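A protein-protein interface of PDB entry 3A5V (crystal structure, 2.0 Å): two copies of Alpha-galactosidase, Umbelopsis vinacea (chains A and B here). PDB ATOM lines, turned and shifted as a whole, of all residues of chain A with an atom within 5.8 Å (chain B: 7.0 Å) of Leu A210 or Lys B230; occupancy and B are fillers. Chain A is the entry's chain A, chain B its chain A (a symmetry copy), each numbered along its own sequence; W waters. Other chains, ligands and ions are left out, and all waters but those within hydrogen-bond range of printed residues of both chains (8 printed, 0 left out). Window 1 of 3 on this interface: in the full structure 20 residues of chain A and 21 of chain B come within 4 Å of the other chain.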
ATOM      1  N   CYS A 131       3.889  37.570  -4.978  1.00  0.00           N
ATOM      2  CA  CYS A 131       3.261  36.439  -5.672  1.00  0.00           C
ATOM      3  C   CYS A 131       2.004  36.842  -6.443  1.00  0.00           C
ATOM      4  O   CYS A 131       1.267  37.723  -6.009  1.00  0.00           O
ATOM      5  CB  CYS A 131       2.921  35.301  -4.702  1.00  0.00           C
ATOM      6  SG  CYS A 131       4.377  34.314  -4.239  1.00  0.00           S
ATOM      7  N   TYR A 132       1.795  36.193  -7.593  1.00  0.00           N
ATOM      8  CA  TYR A 132       0.562  36.299  -8.385  1.00  0.00           C
ATOM      9  C   TYR A 132       0.247  37.733  -8.824  1.00  0.00           C
ATOM     10  O   TYR A 132      -0.889  38.199  -8.709  1.00  0.00           O
ATOM     11  CB  TYR A 132      -0.616  35.601  -7.644  1.00  0.00           C
ATOM     12  CG  TYR A 132      -0.293  34.144  -7.352  1.00  0.00           C
ATOM     13  CD1 TYR A 132      -0.120  33.229  -8.413  1.00  0.00           C
ATOM     14  CD2 TYR A 132      -0.100  33.680  -6.042  1.00  0.00           C
ATOM     15  CE1 TYR A 132       0.193  31.902  -8.179  1.00  0.00           C
ATOM     16  CE2 TYR A 132       0.232  32.329  -5.795  1.00  0.00           C
ATOM     17  CZ  TYR A 132       0.373  31.453  -6.879  1.00  0.00           C
ATOM     18  OH  TYR A 132       0.693  30.121  -6.688  1.00  0.00           O
ATOM     19  N   TRP A 168      11.699  40.503  -3.548  1.00  0.00           N
ATOM     20  CA  TRP A 168      12.819  39.597  -3.740  1.00  0.00           C
ATOM     21  C   TRP A 168      13.920  40.178  -4.635  1.00  0.00           C
ATOM     22  O   TRP A 168      14.673  39.424  -5.250  1.00  0.00           O
ATOM     23  CB  TRP A 168      12.344  38.275  -4.365  1.00  0.00           C
ATOM     24  CG  TRP A 168      10.975  37.749  -3.922  1.00  0.00           C
ATOM     25  CD1 TRP A 168      10.522  37.565  -2.631  1.00  0.00           C
ATOM     26  CD2 TRP A 168       9.916  37.317  -4.787  1.00  0.00           C
ATOM     27  NE1 TRP A 168       9.241  37.048  -2.655  1.00  0.00           N
ATOM     28  CE2 TRP A 168       8.850  36.872  -3.960  1.00  0.00           C
ATOM     29  CE3 TRP A 168       9.773  37.242  -6.186  1.00  0.00           C
ATOM     30  CZ2 TRP A 168       7.651  36.362  -4.486  1.00  0.00           C
ATOM     31  CZ3 TRP A 168       8.574  36.728  -6.712  1.00  0.00           C
ATOM     32  CH2 TRP A 168       7.535  36.285  -5.854  1.00  0.00           C
ATOM     33  N   ALA A 200      16.253  26.095  -7.126  1.00  0.00           N
ATOM     34  CA  ALA A 200      15.168  27.078  -6.915  1.00  0.00           C
ATOM     35  C   ALA A 200      15.706  28.487  -6.627  1.00  0.00           C
ATOM     36  O   ALA A 200      14.945  29.449  -6.627  1.00  0.00           O
ATOM     37  CB  ALA A 200      14.196  26.616  -5.798  1.00  0.00           C
ATOM     38  N   CYS A 201      17.013  28.592  -6.372  1.00  0.00           N
ATOM     39  CA  CYS A 201      17.685  29.897  -6.205  1.00  0.00           C
ATOM     40  C   CYS A 201      18.828  30.013  -7.240  1.00  0.00           C
ATOM     41  O   CYS A 201      20.024  29.965  -6.875  1.00  0.00           O
ATOM     42  CB  CYS A 201      18.199  30.067  -4.771  1.00  0.00           C
ATOM     43  SG  CYS A 201      18.985  31.692  -4.445  1.00  0.00           S
ATOM     44  N   PRO A 202      18.472  30.113  -8.538  1.00  0.00           N
ATOM     45  CA  PRO A 202      19.509  30.054  -9.567  1.00  0.00           C
ATOM     46  C   PRO A 202      20.437  31.273  -9.606  1.00  0.00           C
ATOM     47  O   PRO A 202      21.595  31.139  -9.991  1.00  0.00           O
ATOM     48  CB  PRO A 202      18.702  29.958 -10.873  1.00  0.00           C
ATOM     49  CG  PRO A 202      17.392  30.638 -10.554  1.00  0.00           C
ATOM     50  CD  PRO A 202      17.120  30.263  -9.119  1.00  0.00           C
ATOM     51  N   CYS A 203      19.950  32.449  -9.211  1.00  0.00           N
ATOM     52  CA  CYS A 203      20.746  33.671  -9.373  1.00  0.00           C
ATOM     53  C   CYS A 203      21.849  33.751  -8.327  1.00  0.00           C
ATOM     54  O   CYS A 203      21.623  33.436  -7.164  1.00  0.00           O
ATOM     55  CB  CYS A 203      19.865  34.911  -9.251  1.00  0.00           C
ATOM     56  SG  CYS A 203      18.591  35.033 -10.519  1.00  0.00           S
ATOM     57  N   CYS A 208      18.533  39.697 -11.284  1.00  0.00           N
ATOM     58  CA  CYS A 208      17.820  38.427 -11.239  1.00  0.00           C
ATOM     59  C   CYS A 208      16.369  38.532 -11.694  1.00  0.00           C
ATOM     60  O   CYS A 208      15.632  39.409 -11.240  1.00  0.00           O
ATOM     61  CB  CYS A 208      17.890  37.899  -9.797  1.00  0.00           C
ATOM     62  SG  CYS A 208      17.204  36.262  -9.614  1.00  0.00           S
ATOM     63  N   VAL A 209      15.942  37.635 -12.588  1.00  0.00           N
ATOM     64  CA  VAL A 209      14.531  37.614 -12.990  1.00  0.00           C
ATOM     65  C   VAL A 209      13.742  36.436 -12.382  1.00  0.00           C
ATOM     66  O   VAL A 209      12.544  36.288 -12.638  1.00  0.00           O
ATOM     67  CB  VAL A 209      14.347  37.588 -14.547  1.00  0.00           C
ATOM     68  CG1 VAL A 209      15.023  38.789 -15.194  1.00  0.00           C
ATOM     69  CG2 VAL A 209      14.868  36.314 -15.107  1.00  0.00           C
ATOM     70  N   LEU A 210      14.424  35.589 -11.611  1.00  0.00           N
ATOM     71  CA  LEU A 210      13.763  34.490 -10.897  1.00  0.00           C
ATOM     72  C   LEU A 210      14.417  34.349  -9.530  1.00  0.00           C
ATOM     73  O   LEU A 210      15.356  33.590  -9.348  1.00  0.00           O
ATOM     74  CB  LEU A 210      13.807  33.173 -11.704  1.00  0.00           C
ATOM     75  CG  LEU A 210      13.195  31.900 -11.075  1.00  0.00           C
ATOM     76  CD1 LEU A 210      11.728  32.084 -10.708  1.00  0.00           C
ATOM     77  CD2 LEU A 210      13.350  30.718 -12.030  1.00  0.00           C
ATOM     78  N   ALA A 211      13.925  35.128  -8.567  1.00  0.00           N
ATOM     79  CA  ALA A 211      14.542  35.195  -7.241  1.00  0.00           C
ATOM     80  C   ALA A 211      14.431  33.868  -6.494  1.00  0.00           C
ATOM     81  O   ALA A 211      15.387  33.425  -5.848  1.00  0.00           O
ATOM     82  CB  ALA A 211      13.907  36.320  -6.430  1.00  0.00           C
ATOM     83  N   GLY A 212      13.266  33.240  -6.594  1.00  0.00           N
ATOM     84  CA  GLY A 212      13.055  31.911  -6.023  1.00  0.00           C
ATOM     85  C   GLY A 212      13.159  31.858  -4.499  1.00  0.00           C
ATOM     86  O   GLY A 212      12.822  32.818  -3.794  1.00  0.00           O
ATOM     87  N   PRO B 173       6.231  32.759 -17.907  1.00  0.00           N
ATOM     88  CA  PRO B 173       4.814  32.409 -17.686  1.00  0.00           C
ATOM     89  C   PRO B 173       4.563  31.739 -16.323  1.00  0.00           C
ATOM     90  O   PRO B 173       3.458  31.845 -15.811  1.00  0.00           O
ATOM     91  CB  PRO B 173       4.493  31.449 -18.822  1.00  0.00           C
ATOM     92  CG  PRO B 173       5.864  30.849 -19.231  1.00  0.00           C
ATOM     93  CD  PRO B 173       6.825  32.001 -19.030  1.00  0.00           C
ATOM     94  N   TRP B 174       5.581  31.092 -15.743  1.00  0.00           N
ATOM     95  CA  TRP B 174       5.490  30.530 -14.377  1.00  0.00           C
ATOM     96  C   TRP B 174       5.175  31.605 -13.321  1.00  0.00           C
ATOM     97  O   TRP B 174       4.694  31.283 -12.231  1.00  0.00           O
ATOM     98  CB  TRP B 174       6.775  29.748 -14.002  1.00  0.00           C
ATOM     99  CG  TRP B 174       8.031  30.491 -14.369  1.00  0.00           C
ATOM    100  CD1 TRP B 174       8.650  31.479 -13.644  1.00  0.00           C
ATOM    101  CD2 TRP B 174       8.777  30.354 -15.586  1.00  0.00           C
ATOM    102  NE1 TRP B 174       9.754  31.941 -14.333  1.00  0.00           N
ATOM    103  CE2 TRP B 174       9.852  31.268 -15.525  1.00  0.00           C
ATOM    104  CE3 TRP B 174       8.654  29.519 -16.714  1.00  0.00           C
ATOM    105  CZ2 TRP B 174      10.814  31.377 -16.552  1.00  0.00           C
ATOM    106  CZ3 TRP B 174       9.601  29.624 -17.738  1.00  0.00           C
ATOM    107  CH2 TRP B 174      10.668  30.556 -17.652  1.00  0.00           C
ATOM    108  N   ASN B 175       5.462  32.873 -13.649  1.00  0.00           N
ATOM    109  CA  ASN B 175       5.057  34.028 -12.834  1.00  0.00           C
ATOM    110  C   ASN B 175       3.724  34.628 -13.312  1.00  0.00           C
ATOM    111  O   ASN B 175       2.801  34.801 -12.517  1.00  0.00           O
ATOM    112  CB  ASN B 175       6.137  35.137 -12.839  1.00  0.00           C
ATOM    113  CG  ASN B 175       7.510  34.639 -12.388  1.00  0.00           C
ATOM    114  OD1 ASN B 175       7.649  33.938 -11.371  1.00  0.00           O
ATOM    115  ND2 ASN B 175       8.544  35.020 -13.145  1.00  0.00           N
ATOM    116  N   SER B 178       0.019  32.037 -14.156  1.00  0.00           N
ATOM    117  CA  SER B 178      -0.367  30.969 -13.230  1.00  0.00           C
ATOM    118  C   SER B 178      -1.825  31.023 -12.778  1.00  0.00           C
ATOM    119  O   SER B 178      -2.390  29.994 -12.416  1.00  0.00           O
ATOM    120  CB  SER B 178       0.564  30.937 -12.014  1.00  0.00           C
ATOM    121  OG  SER B 178       0.662  32.223 -11.451  1.00  0.00           O
ATOM    122  N   TRP B 184       1.836  25.961 -19.004  1.00  0.00           N
ATOM    123  CA  TRP B 184       2.639  26.851 -19.841  1.00  0.00           C
ATOM    124  C   TRP B 184       3.928  26.140 -20.236  1.00  0.00           C
ATOM    125  O   TRP B 184       4.667  25.642 -19.381  1.00  0.00           O
ATOM    126  CB  TRP B 184       2.929  28.199 -19.137  1.00  0.00           C
ATOM    127  CG  TRP B 184       3.225  28.024 -17.691  1.00  0.00           C
ATOM    128  CD1 TRP B 184       4.451  27.747 -17.123  1.00  0.00           C
ATOM    129  CD2 TRP B 184       2.272  28.023 -16.621  1.00  0.00           C
ATOM    130  NE1 TRP B 184       4.306  27.599 -15.760  1.00  0.00           N
ATOM    131  CE2 TRP B 184       2.984  27.761 -15.426  1.00  0.00           C
ATOM    132  CE3 TRP B 184       0.880  28.231 -16.555  1.00  0.00           C
ATOM    133  CZ2 TRP B 184       2.353  27.716 -14.168  1.00  0.00           C
ATOM    134  CZ3 TRP B 184       0.249  28.167 -15.304  1.00  0.00           C
ATOM    135  CH2 TRP B 184       0.988  27.911 -14.129  1.00  0.00           C
ATOM    136  N   TYR B 206      16.428  28.890 -17.860  1.00  0.00           N
ATOM    137  CA  TYR B 206      15.044  29.392 -17.850  1.00  0.00           C
ATOM    138  C   TYR B 206      14.947  30.801 -18.428  1.00  0.00           C
ATOM    139  O   TYR B 206      13.890  31.197 -18.915  1.00  0.00           O
ATOM    140  CB  TYR B 206      14.461  29.395 -16.403  1.00  0.00           C
ATOM    141  CG  TYR B 206      15.184  30.417 -15.540  1.00  0.00           C
ATOM    142  CD1 TYR B 206      16.349  30.073 -14.862  1.00  0.00           C
ATOM    143  CD2 TYR B 206      14.744  31.750 -15.476  1.00  0.00           C
ATOM    144  CE1 TYR B 206      17.061  31.015 -14.113  1.00  0.00           C
ATOM    145  CE2 TYR B 206      15.449  32.702 -14.739  1.00  0.00           C
ATOM    146  CZ  TYR B 206      16.595  32.319 -14.056  1.00  0.00           C
ATOM    147  OH  TYR B 206      17.297  33.247 -13.335  1.00  0.00           O
ATOM    148  N   ASP B 207      16.042  31.566 -18.355  1.00  0.00           N
ATOM    149  CA  ASP B 207      16.036  32.963 -18.786  1.00  0.00           C
ATOM    150  C   ASP B 207      16.452  33.112 -20.267  1.00  0.00           C
ATOM    151  O   ASP B 207      17.636  33.069 -20.614  1.00  0.00           O
ATOM    152  CB  ASP B 207      16.945  33.789 -17.869  1.00  0.00           C
ATOM    153  CG  ASP B 207      16.763  35.289 -18.061  1.00  0.00           C
ATOM    154  OD1 ASP B 207      15.829  35.718 -18.774  1.00  0.00           O
ATOM    155  OD2 ASP B 207      17.574  36.038 -17.496  1.00  0.00           O
ATOM    156  N   LYS B 223      16.491  23.427 -17.699  1.00  0.00           N
ATOM    157  CA  LYS B 223      15.582  24.592 -17.577  1.00  0.00           C
ATOM    158  C   LYS B 223      14.450  24.358 -16.586  1.00  0.00           C
ATOM    159  O   LYS B 223      14.117  25.233 -15.780  1.00  0.00           O
ATOM    160  CB  LYS B 223      14.990  24.970 -18.951  1.00  0.00           C
ATOM    161  CG  LYS B 223      16.050  25.502 -19.922  1.00  0.00           C
ATOM    162  CD  LYS B 223      15.566  25.493 -21.382  1.00  0.00           C
ATOM    163  CE  LYS B 223      16.622  26.177 -22.264  1.00  0.00           C
ATOM    164  NZ  LYS B 223      16.405  25.917 -23.740  1.00  0.00           N
ATOM    165  N   ALA B 226      14.661  24.854 -12.503  1.00  0.00           N
ATOM    166  CA  ALA B 226      14.562  26.210 -11.947  1.00  0.00           C
ATOM    167  C   ALA B 226      13.125  26.641 -11.667  1.00  0.00           C
ATOM    168  O   ALA B 226      12.891  27.431 -10.767  1.00  0.00           O
ATOM    169  CB  ALA B 226      15.244  27.264 -12.882  1.00  0.00           C
ATOM    170  N   VAL B 227      12.163  26.122 -12.428  1.00  0.00           N
ATOM    171  CA  VAL B 227      10.790  26.661 -12.373  1.00  0.00           C
ATOM    172  C   VAL B 227       9.757  25.738 -11.708  1.00  0.00           C
ATOM    173  O   VAL B 227       8.610  26.155 -11.475  1.00  0.00           O
ATOM    174  CB  VAL B 227      10.305  27.175 -13.770  1.00  0.00           C
ATOM    175  CG1 VAL B 227      11.261  28.271 -14.288  1.00  0.00           C
ATOM    176  CG2 VAL B 227      10.212  26.025 -14.820  1.00  0.00           C
ATOM    177  N   SER B 228      10.168  24.511 -11.388  1.00  0.00           N
ATOM    178  CA  SER B 228       9.313  23.532 -10.682  1.00  0.00           C
ATOM    179  C   SER B 228       8.668  24.152  -9.458  1.00  0.00           C
ATOM    180  O   SER B 228       7.504  23.873  -9.143  1.00  0.00           O
ATOM    181  CB  SER B 228      10.136  22.309 -10.236  1.00  0.00           C
ATOM    182  OG  SER B 228      10.476  21.490 -11.343  1.00  0.00           O
ATOM    183  N   GLN B 229       9.424  25.018  -8.777  1.00  0.00           N
ATOM    184  CA  GLN B 229       8.936  25.678  -7.560  1.00  0.00           C
ATOM    185  C   GLN B 229       7.591  26.432  -7.756  1.00  0.00           C
ATOM    186  O   GLN B 229       6.897  26.715  -6.773  1.00  0.00           O
ATOM    187  CB  GLN B 229       9.994  26.672  -7.037  1.00  0.00           C
ATOM    188  CG  GLN B 229      10.355  27.772  -8.053  1.00  0.00           C
ATOM    189  CD  GLN B 229      11.420  28.721  -7.510  1.00  0.00           C
ATOM    190  OE1 GLN B 229      11.240  29.312  -6.450  1.00  0.00           O
ATOM    191  NE2 GLN B 229      12.519  28.874  -8.241  1.00  0.00           N
ATOM    192  N   LYS B 230       7.254  26.795  -8.998  1.00  0.00           N
ATOM    193  CA  LYS B 230       6.070  27.614  -9.254  1.00  0.00           C
ATOM    194  C   LYS B 230       4.816  26.791  -9.545  1.00  0.00           C
ATOM    195  O   LYS B 230       3.704  27.333  -9.533  1.00  0.00           O
ATOM    196  CB  LYS B 230       6.304  28.610 -10.421  1.00  0.00           C
ATOM    197  CG  LYS B 230       7.442  29.637 -10.205  1.00  0.00           C
ATOM    198  CD  LYS B 230       7.178  30.576  -9.046  1.00  0.00           C
ATOM    199  CE  LYS B 230       8.399  31.457  -8.815  1.00  0.00           C
ATOM    200  NZ  LYS B 230       8.132  32.449  -7.737  1.00  0.00           N
ATOM    201  N   ALA B 231       4.999  25.498  -9.811  1.00  0.00           N
ATOM    202  CA  ALA B 231       3.917  24.618 -10.262  1.00  0.00           C
ATOM    203  C   ALA B 231       2.939  24.354  -9.130  1.00  0.00           C
ATOM    204  O   ALA B 231       3.361  24.178  -7.989  1.00  0.00           O
ATOM    205  CB  ALA B 231       4.497  23.290 -10.742  1.00  0.00           C
ATOM    206  N   ARG B 232       1.647  24.291  -9.454  1.00  0.00           N
ATOM    207  CA  ARG B 232       0.586  24.043  -8.456  1.00  0.00           C
ATOM    208  C   ARG B 232      -0.550  23.275  -9.148  1.00  0.00           C
ATOM    209  O   ARG B 232      -0.659  23.298 -10.375  1.00  0.00           O
ATOM    210  CB  ARG B 232      -0.024  25.360  -7.940  1.00  0.00           C
ATOM    211  CG  ARG B 232       0.947  26.369  -7.271  1.00  0.00           C
ATOM    212  CD  ARG B 232       1.367  25.943  -5.852  1.00  0.00           C
ATOM    213  NE  ARG B 232       2.273  26.941  -5.275  1.00  0.00           N
ATOM    214  CZ  ARG B 232       3.610  26.940  -5.407  1.00  0.00           C
ATOM    215  NH1 ARG B 232       4.242  25.958  -6.055  1.00  0.00           N
ATOM    216  NH2 ARG B 232       4.333  27.914  -4.855  1.00  0.00           N
ATOM    217  N   GLY B 235      -2.157  24.455 -12.539  1.00  0.00           N
ATOM    218  CA  GLY B 235      -1.225  25.432 -13.136  1.00  0.00           C
ATOM    219  C   GLY B 235       0.186  24.849 -13.217  1.00  0.00           C
ATOM    220  O   GLY B 235       1.006  25.022 -12.300  1.00  0.00           O
ATOM    221  N   TRP B 236       0.471  24.201 -14.337  1.00  0.00           N
ATOM    222  CA  TRP B 236       1.660  23.350 -14.482  1.00  0.00           C
ATOM    223  C   TRP B 236       2.706  23.898 -15.451  1.00  0.00           C
ATOM    224  O   TRP B 236       2.353  24.465 -16.476  1.00  0.00           O
ATOM    225  CB  TRP B 236       1.228  21.972 -15.022  1.00  0.00           C
ATOM    226  CG  TRP B 236       0.138  21.338 -14.190  1.00  0.00           C
ATOM    227  CD1 TRP B 236      -1.166  21.186 -14.533  1.00  0.00           C
ATOM    228  CD2 TRP B 236       0.278  20.805 -12.876  1.00  0.00           C
ATOM    229  NE1 TRP B 236      -1.861  20.584 -13.518  1.00  0.00           N
ATOM    230  CE2 TRP B 236      -1.009  20.352 -12.473  1.00  0.00           C
ATOM    231  CE3 TRP B 236       1.353  20.699 -11.979  1.00  0.00           C
ATOM    232  CZ2 TRP B 236      -1.243  19.759 -11.227  1.00  0.00           C
ATOM    233  CZ3 TRP B 236       1.123  20.114 -10.719  1.00  0.00           C
ATOM    234  CH2 TRP B 236      -0.167  19.637 -10.363  1.00  0.00           C
ATOM    235  N   ASN B 237       3.979  23.609 -15.176  1.00  0.00           N
ATOM    236  CA  ASN B 237       5.051  23.754 -16.179  1.00  0.00           C
ATOM    237  C   ASN B 237       4.913  22.645 -17.224  1.00  0.00           C
ATOM    238  O   ASN B 237       4.658  21.492 -16.871  1.00  0.00           O
ATOM    239  CB  ASN B 237       6.444  23.682 -15.506  1.00  0.00           C
ATOM    240  CG  ASN B 237       6.642  24.793 -14.467  1.00  0.00           C
ATOM    241  OD1 ASN B 237       6.423  25.978 -14.752  1.00  0.00           O
ATOM    242  ND2 ASN B 237       7.046  24.408 -13.257  1.00  0.00           N
ATOM    243  N   PRO B 301       5.962  18.831  -7.833  1.00  0.00           N
ATOM    244  CA  PRO B 301       7.084  18.326  -8.628  1.00  0.00           C
ATOM    245  C   PRO B 301       8.223  17.819  -7.734  1.00  0.00           C
ATOM    246  O   PRO B 301       8.433  18.343  -6.625  1.00  0.00           O
ATOM    247  CB  PRO B 301       7.576  19.573  -9.398  1.00  0.00           C
ATOM    248  CG  PRO B 301       6.420  20.500  -9.423  1.00  0.00           C
ATOM    249  CD  PRO B 301       5.712  20.264  -8.087  1.00  0.00           C
HETATM  250  O   HOH W   1       0.488  29.095  -4.234  1.00  0.00           O
HETATM  251  O   HOH W   2      11.235  34.421 -14.031  1.00  0.00           O
HETATM  252  O   HOH W   3      10.605  34.001  -7.474  1.00  0.00           O
HETATM  253  O   HOH W   4       6.773  32.028  -5.631  1.00  0.00           O
HETATM  254  O   HOH W   5       3.512  36.753 -10.298  1.00  0.00           O
HETATM  255  O   HOH W   6      17.679  35.769 -13.907  1.00  0.00           O
HETATM  256  O   HOH W   7       3.058  29.687  -8.362  1.00  0.00           O
HETATM  257  O   HOH W   8      19.961  32.745 -12.903  1.00  0.00           O
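Of the 19 printed residues of chain B, 8 touch a printed residue of chain A.
Hydrophobic or aromatic side chains of chain B that line the printed part of chain A: Tyr B206 and Val B227.
Of the 12 printed residues of chain A, 7 touch a printed residue of chain B.
Hydrophobic or aromatic side chains of chain A that line the printed part of chain B: Tyr A132, Ala A200, Pro A202, Val A209 and Leu A210.
Among the printed residues, 12 pairs touch across the chains.
Water W4 bridges NZ of Lys B230 (2.5 Å) and SG of Cys A131 (3.6 Å).
Water W6 lies within hydrogen-bond range of OH of Tyr B206 (2.6 Å), N of Val A209 (2.9 Å) and SG of Cys A203 (3.6 Å).
Water W1 bridges the side-chain hydroxyl (OH) of Tyr A132 (2.7 Å) and the guanidinium group (NE) of Arg B232 (3.0 Å).
Water W7 bridges the backbone carbonyl oxygen of Lys B230 (2.7 Å) and the side-chain hydroxyl of Tyr A132 (2.9 Å).
Water W8 bridges the side-chain hydroxyl (OH) of Tyr B206 and the side-chain sulfur (SG) of Cys A203.
Water W5 lies within hydrogen-bond range of O of Asn B175 and N of Tyr A132.
No position is printed for both chains.
Of the 12 pairs that touch across the chains among the printed residues, none has its exchanged pair printed and touching as well.
O of Ala A200 lies within hydrogen-bond range of NE2 of Gln B229 (3.0 Å).
SG of Cys A203 is in hydrogen-bond range of OH of Tyr B206, at 3.6 Å.
SG of Cys A208 sits close to N of Leu A210 (3.5 Å).
O of Ala B226 sits at hydrogen-bond distance from NE2 of Gln B229.
The side-chain sulfur (SG) of Cys A203 forms a disulfide with the side-chain sulfur (SG) of Cys A208 (2.1 Å).
O of Val B227 sits at hydrogen-bond distance from ND2 of Asn B237 (2.9 Å).
The guanidinium group of Arg B232 sits at hydrogen-bond distance from the backbone carbonyl oxygen of Gln B229 (2.9 Å).
Ser B178 touches Tyr A132 (OG to CD1, 3.3 Å).
Arg B232 touches Tyr A132.
Pro A202 touches Tyr B206.
Tyr B206 touches Val A209 (CE2 to CG2, 3.7 Å).
Val A209 touches Asp B207 (CG2 to OD2, 3.6 Å).
CB of Leu A210 touches CE2 of Tyr B206 (3.5 Å).
Ala B226 touches Leu A210 (O to CD2, 3.6 Å).
CG1 of Val B227 touches CD2 of Leu A210, 3.9 Å away.
CD1 of Leu A210 touches CE of Lys B230 (3.9 Å).
Gly A212 touches Gln B229 (CA to OE1, 3.2 Å).
Printed residues of chain B within 4 Å of Pro A202: Tyr B206 (3.6 Å).
Of the printed residues of chain B, Cys A203 touches Tyr B206 (3.6 Å).
Leu A210 touches just these residues of chain B: Tyr B206 (3.5 Å), Ala B226 (3.6 Å), Val B227 (3.9 Å) and Lys B230 (3.9 Å).
Ala A211 touches none of the printed residues of chain B.
Printed residues of chain A within 4 Å of Val B227: Leu A210.
Pro B301 touches none of the printed residues of chain A.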
